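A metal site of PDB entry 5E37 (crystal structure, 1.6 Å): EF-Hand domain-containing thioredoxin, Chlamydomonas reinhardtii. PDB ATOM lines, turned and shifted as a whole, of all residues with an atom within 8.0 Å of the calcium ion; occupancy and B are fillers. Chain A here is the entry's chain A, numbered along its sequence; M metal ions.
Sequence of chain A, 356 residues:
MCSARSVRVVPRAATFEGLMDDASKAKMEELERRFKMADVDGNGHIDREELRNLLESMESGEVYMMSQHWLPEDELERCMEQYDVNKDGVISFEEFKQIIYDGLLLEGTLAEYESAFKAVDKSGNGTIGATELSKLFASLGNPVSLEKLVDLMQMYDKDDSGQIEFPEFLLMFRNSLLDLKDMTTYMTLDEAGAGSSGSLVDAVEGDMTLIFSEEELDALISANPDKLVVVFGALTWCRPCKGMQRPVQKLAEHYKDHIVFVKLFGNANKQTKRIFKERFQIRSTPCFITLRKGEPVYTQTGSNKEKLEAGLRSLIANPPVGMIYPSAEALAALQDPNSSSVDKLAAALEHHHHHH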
ATOM      1  N   THR A 127     -16.178  32.296  22.972  1.00  0.00           N
ATOM      2  CA  THR A 127     -16.959  31.901  21.766  1.00  0.00           C
ATOM      3  C   THR A 127     -16.087  31.099  20.846  1.00  0.00           C
ATOM      4  O   THR A 127     -14.873  31.144  20.941  1.00  0.00           O
ATOM      5  CB  THR A 127     -17.541  33.035  20.945  1.00  0.00           C
ATOM      6  OG1 THR A 127     -16.506  33.806  20.355  1.00  0.00           O
ATOM      7  CG2 THR A 127     -18.319  33.988  21.842  1.00  0.00           C
ATOM      8  N   ILE A 128     -16.694  30.207  20.080  1.00  0.00           N
ATOM      9  CA  ILE A 128     -15.942  29.273  19.164  1.00  0.00           C
ATOM     10  C   ILE A 128     -15.964  29.772  17.731  1.00  0.00           C
ATOM     11  O   ILE A 128     -17.041  29.926  17.180  1.00  0.00           O
ATOM     12  CB  ILE A 128     -16.488  27.839  19.265  1.00  0.00           C
ATOM     13  CG1 ILE A 128     -16.248  27.260  20.678  1.00  0.00           C
ATOM     14  CG2 ILE A 128     -15.935  26.964  18.160  1.00  0.00           C
ATOM     15  CD1 ILE A 128     -17.014  26.010  20.959  1.00  0.00           C
ATOM     16  N   MET A 153     -20.965  26.238   9.743  1.00  0.00           N
ATOM     17  CA  MET A 153     -21.421  27.553  10.210  1.00  0.00           C
ATOM     18  C   MET A 153     -22.808  27.901   9.786  1.00  0.00           C
ATOM     19  O   MET A 153     -23.559  28.485  10.591  1.00  0.00           O
ATOM     20  CB  MET A 153     -20.435  28.650   9.754  1.00  0.00           C
ATOM     21  CG  MET A 153     -19.057  28.473  10.378  1.00  0.00           C
ATOM     22  SD  MET A 153     -18.979  28.659  12.172  1.00  0.00           S
ATOM     23  CE  MET A 153     -19.165  30.435  12.317  1.00  0.00           C
ATOM     24  N   TYR A 156     -25.084  25.764  12.176  1.00  0.00           N
ATOM     25  CA  TYR A 156     -25.053  25.997  13.568  1.00  0.00           C
ATOM     26  C   TYR A 156     -24.938  27.417  14.076  1.00  0.00           C
ATOM     27  O   TYR A 156     -25.377  27.720  15.205  1.00  0.00           O
ATOM     28  CB  TYR A 156     -23.967  25.120  14.173  1.00  0.00           C
ATOM     29  CG  TYR A 156     -24.315  23.652  14.127  1.00  0.00           C
ATOM     30  CD1 TYR A 156     -25.285  23.137  14.921  1.00  0.00           C
ATOM     31  CD2 TYR A 156     -23.841  22.845  13.107  1.00  0.00           C
ATOM     32  CE1 TYR A 156     -25.695  21.826  14.816  1.00  0.00           C
ATOM     33  CE2 TYR A 156     -24.166  21.501  13.027  1.00  0.00           C
ATOM     34  CZ  TYR A 156     -25.118  21.018  13.840  1.00  0.00           C
ATOM     35  OH  TYR A 156     -25.573  19.702  13.746  1.00  0.00           O
ATOM     36  N   ASP A 157     -24.343  28.297  13.233  1.00  0.00           N
ATOM     37  CA  ASP A 157     -24.300  29.707  13.560  1.00  0.00           C
ATOM     38  C   ASP A 157     -25.616  30.349  13.106  1.00  0.00           C
ATOM     39  O   ASP A 157     -25.663  31.144  12.181  1.00  0.00           O
ATOM     40  CB  ASP A 157     -23.072  30.397  12.923  1.00  0.00           C
ATOM     41  CG  ASP A 157     -23.023  31.854  13.234  1.00  0.00           C
ATOM     42  OD1 ASP A 157     -23.565  32.358  14.224  1.00  0.00           O
ATOM     43  OD2 ASP A 157     -22.457  32.634  12.452  1.00  0.00           O
ATOM     44  N   LYS A 158     -26.669  30.078  13.863  1.00  0.00           N
ATOM     45  CA  LYS A 158     -27.992  30.431  13.431  1.00  0.00           C
ATOM     46  C   LYS A 158     -28.297  31.893  13.588  1.00  0.00           C
ATOM     47  O   LYS A 158     -29.286  32.343  13.021  1.00  0.00           O
ATOM     48  CB  LYS A 158     -29.042  29.747  14.275  1.00  0.00           C
ATOM     49  CG  LYS A 158     -28.824  28.319  14.539  1.00  0.00           C
ATOM     50  CD  LYS A 158     -29.143  27.539  13.354  1.00  0.00           C
ATOM     51  CE  LYS A 158     -29.692  26.178  13.827  1.00  0.00           C
ATOM     52  NZ  LYS A 158     -30.348  25.434  12.725  1.00  0.00           N
ATOM     53  N   ASP A 159     -27.561  32.650  14.395  1.00  0.00           N
ATOM     54  CA  ASP A 159     -27.783  34.068  14.494  1.00  0.00           C
ATOM     55  C   ASP A 159     -26.818  34.920  13.647  1.00  0.00           C
ATOM     56  O   ASP A 159     -26.711  36.159  13.808  1.00  0.00           O
ATOM     57  CB  ASP A 159     -27.805  34.479  15.971  1.00  0.00           C
ATOM     58  CG  ASP A 159     -26.493  34.326  16.658  1.00  0.00           C
ATOM     59  OD1 ASP A 159     -25.455  33.842  16.142  1.00  0.00           O
ATOM     60  OD2 ASP A 159     -26.373  34.761  17.800  1.00  0.00           O
ATOM     61  N   ASP A 160     -26.030  34.246  12.802  1.00  0.00           N
ATOM     62  CA  ASP A 160     -25.084  34.952  11.921  1.00  0.00           C
ATOM     63  C   ASP A 160     -24.163  35.870  12.672  1.00  0.00           C
ATOM     64  O   ASP A 160     -23.770  36.932  12.148  1.00  0.00           O
ATOM     65  CB  ASP A 160     -25.854  35.676  10.821  1.00  0.00           C
ATOM     66  CG  ASP A 160     -26.476  34.745   9.850  1.00  0.00           C
ATOM     67  OD1 ASP A 160     -26.417  33.511  10.037  1.00  0.00           O
ATOM     68  OD2 ASP A 160     -27.026  35.204   8.863  1.00  0.00           O
ATOM     69  N   SER A 161     -23.718  35.445  13.848  1.00  0.00           N
ATOM     70  CA  SER A 161     -22.686  36.155  14.615  1.00  0.00           C
ATOM     71  C   SER A 161     -21.254  35.969  14.132  1.00  0.00           C
ATOM     72  O   SER A 161     -20.353  36.709  14.543  1.00  0.00           O
ATOM     73  CB  SER A 161     -22.763  35.848  16.068  1.00  0.00           C
ATOM     74  OG  SER A 161     -22.325  34.546  16.332  1.00  0.00           O
ATOM     75  N   GLY A 162     -21.066  34.920  13.323  1.00  0.00           N
ATOM     76  CA  GLY A 162     -19.775  34.462  12.912  1.00  0.00           C
ATOM     77  C   GLY A 162     -19.034  33.682  13.952  1.00  0.00           C
ATOM     78  O   GLY A 162     -17.890  33.318  13.701  1.00  0.00           O
ATOM     79  N   GLN A 163     -19.694  33.322  15.072  1.00  0.00           N
ATOM     80  CA  GLN A 163     -19.135  32.482  16.090  1.00  0.00           C
ATOM     81  C   GLN A 163     -20.186  31.489  16.536  1.00  0.00           C
ATOM     82  O   GLN A 163     -21.427  31.702  16.384  1.00  0.00           O
ATOM     83  CB  GLN A 163     -18.743  33.324  17.324  1.00  0.00           C
ATOM     84  CG  GLN A 163     -17.660  34.356  17.098  1.00  0.00           C
ATOM     85  CD  GLN A 163     -16.286  33.759  16.967  1.00  0.00           C
ATOM     86  OE1 GLN A 163     -15.810  33.134  17.890  1.00  0.00           O
ATOM     87  NE2 GLN A 163     -15.633  34.009  15.852  1.00  0.00           N
ATOM     88  N   ILE A 164     -19.691  30.404  17.079  1.00  0.00           N
ATOM     89  CA  ILE A 164     -20.605  29.425  17.772  1.00  0.00           C
ATOM     90  C   ILE A 164     -20.618  29.796  19.247  1.00  0.00           C
ATOM     91  O   ILE A 164     -19.602  29.675  19.934  1.00  0.00           O
ATOM     92  CB  ILE A 164     -20.117  28.010  17.546  1.00  0.00           C
ATOM     93  CG1 ILE A 164     -20.046  27.632  16.044  1.00  0.00           C
ATOM     94  CG2 ILE A 164     -20.962  26.962  18.286  1.00  0.00           C
ATOM     95  CD1 ILE A 164     -21.300  27.791  15.286  1.00  0.00           C
ATOM     96  N   GLU A 165     -21.756  30.305  19.674  1.00  0.00           N
ATOM     97  CA  GLU A 165     -21.932  30.583  21.126  1.00  0.00           C
ATOM     98  C   GLU A 165     -22.422  29.256  21.794  1.00  0.00           C
ATOM     99  O   GLU A 165     -22.883  28.327  21.139  1.00  0.00           O
ATOM    100  CB  GLU A 165     -22.862  31.758  21.351  1.00  0.00           C
ATOM    101  CG  GLU A 165     -22.303  33.070  20.825  1.00  0.00           C
ATOM    102  CD  GLU A 165     -22.584  33.362  19.366  1.00  0.00           C
ATOM    103  OE1 GLU A 165     -23.568  32.898  18.788  1.00  0.00           O
ATOM    104  OE2 GLU A 165     -21.722  34.099  18.803  1.00  0.00           O
ATOM    105  N   PHE A 166     -22.341  29.262  23.109  1.00  0.00           N
ATOM    106  CA  PHE A 166     -22.795  28.076  23.866  1.00  0.00           C
ATOM    107  C   PHE A 166     -24.092  27.426  23.454  1.00  0.00           C
ATOM    108  O   PHE A 166     -24.141  26.210  23.271  1.00  0.00           O
ATOM    109  CB  PHE A 166     -22.731  28.340  25.344  1.00  0.00           C
ATOM    110  CG  PHE A 166     -22.907  27.124  26.181  1.00  0.00           C
ATOM    111  CD1 PHE A 166     -21.916  26.191  26.264  1.00  0.00           C
ATOM    112  CD2 PHE A 166     -24.101  26.891  26.847  1.00  0.00           C
ATOM    113  CE1 PHE A 166     -22.056  25.062  27.095  1.00  0.00           C
ATOM    114  CE2 PHE A 166     -24.264  25.750  27.644  1.00  0.00           C
ATOM    115  CZ  PHE A 166     -23.219  24.858  27.764  1.00  0.00           C
ATOM    116  N   PRO A 167     -25.175  28.138  23.332  1.00  0.00           N
ATOM    117  CA  PRO A 167     -26.430  27.474  22.911  1.00  0.00           C
ATOM    118  C   PRO A 167     -26.420  26.851  21.579  1.00  0.00           C
ATOM    119  O   PRO A 167     -27.123  25.877  21.334  1.00  0.00           O
ATOM    120  CB  PRO A 167     -27.483  28.596  22.909  1.00  0.00           C
ATOM    121  CG  PRO A 167     -26.819  29.723  23.433  1.00  0.00           C
ATOM    122  CD  PRO A 167     -25.376  29.553  23.562  1.00  0.00           C
ATOM    123  N   GLU A 168     -25.642  27.400  20.643  1.00  0.00           N
ATOM    124  CA  GLU A 168     -25.460  26.757  19.406  1.00  0.00           C
ATOM    125  C   GLU A 168     -24.586  25.513  19.449  1.00  0.00           C
ATOM    126  O   GLU A 168     -24.858  24.516  18.766  1.00  0.00           O
ATOM    127  CB  GLU A 168     -24.856  27.809  18.424  1.00  0.00           C
ATOM    128  CG  GLU A 168     -25.715  29.028  18.139  1.00  0.00           C
ATOM    129  CD  GLU A 168     -25.013  30.147  17.324  1.00  0.00           C
ATOM    130  OE1 GLU A 168     -23.774  30.222  17.357  1.00  0.00           O
ATOM    131  OE2 GLU A 168     -25.803  31.001  16.853  1.00  0.00           O
ATOM    132  N   PHE A 169     -23.538  25.543  20.287  1.00  0.00           N
ATOM    133  CA  PHE A 169     -22.695  24.343  20.555  1.00  0.00           C
ATOM    134  C   PHE A 169     -23.545  23.239  21.043  1.00  0.00           C
ATOM    135  O   PHE A 169     -23.371  22.140  20.591  1.00  0.00           O
ATOM    136  CB  PHE A 169     -21.606  24.759  21.506  1.00  0.00           C
ATOM    137  CG  PHE A 169     -20.596  23.728  21.838  1.00  0.00           C
ATOM    138  CD1 PHE A 169     -19.616  23.386  20.933  1.00  0.00           C
ATOM    139  CD2 PHE A 169     -20.514  23.207  23.143  1.00  0.00           C
ATOM    140  CE1 PHE A 169     -18.617  22.522  21.298  1.00  0.00           C
ATOM    141  CE2 PHE A 169     -19.526  22.355  23.513  1.00  0.00           C
ATOM    142  CZ  PHE A 169     -18.547  22.003  22.610  1.00  0.00           C
HETATM  143 CA    CA M   1     -23.691  32.427  16.520  1.00  0.00          CA
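OD1 of Asp 159 binds the calcium ion (2.3 Å).
The side-chain carboxylate (OD1) of Asp 157 is bound to the calcium ion, at 2.3 Å.
OE1 of Glu 165 is bound to the calcium ion (2.3 Å).
The side-chain carboxylate (OE1) of Glu 168 is bound to the calcium ion (2.4 Å).
The calcium ion is bound by O of Gln 163.
The calcium ion is bound by the side-chain hydroxyl (OG) of Ser 161, at 2.5 Å.
OE2 of Glu 168 is bound to the calcium ion.
The calcium ion has seven donor atoms within binding distance.
The side-chain amide oxygen of Gln 163 is in hydrogen-bond range of the side-chain hydroxyl of Thr 127 (2.6 Å).
N of Asp 160 lies close to OD1 of Asp 157 (3.4 Å).
OE2 of Glu 168 sits close to N of Lys 158, 3.2 Å away.
The backbone NH (N) of Gly 162 is in hydrogen-bond range of the side-chain carboxylate (OD2) of Asp 157 (2.8 Å).
Of the 17 residues printed, 6 come within 4 Å of the calcium ion.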
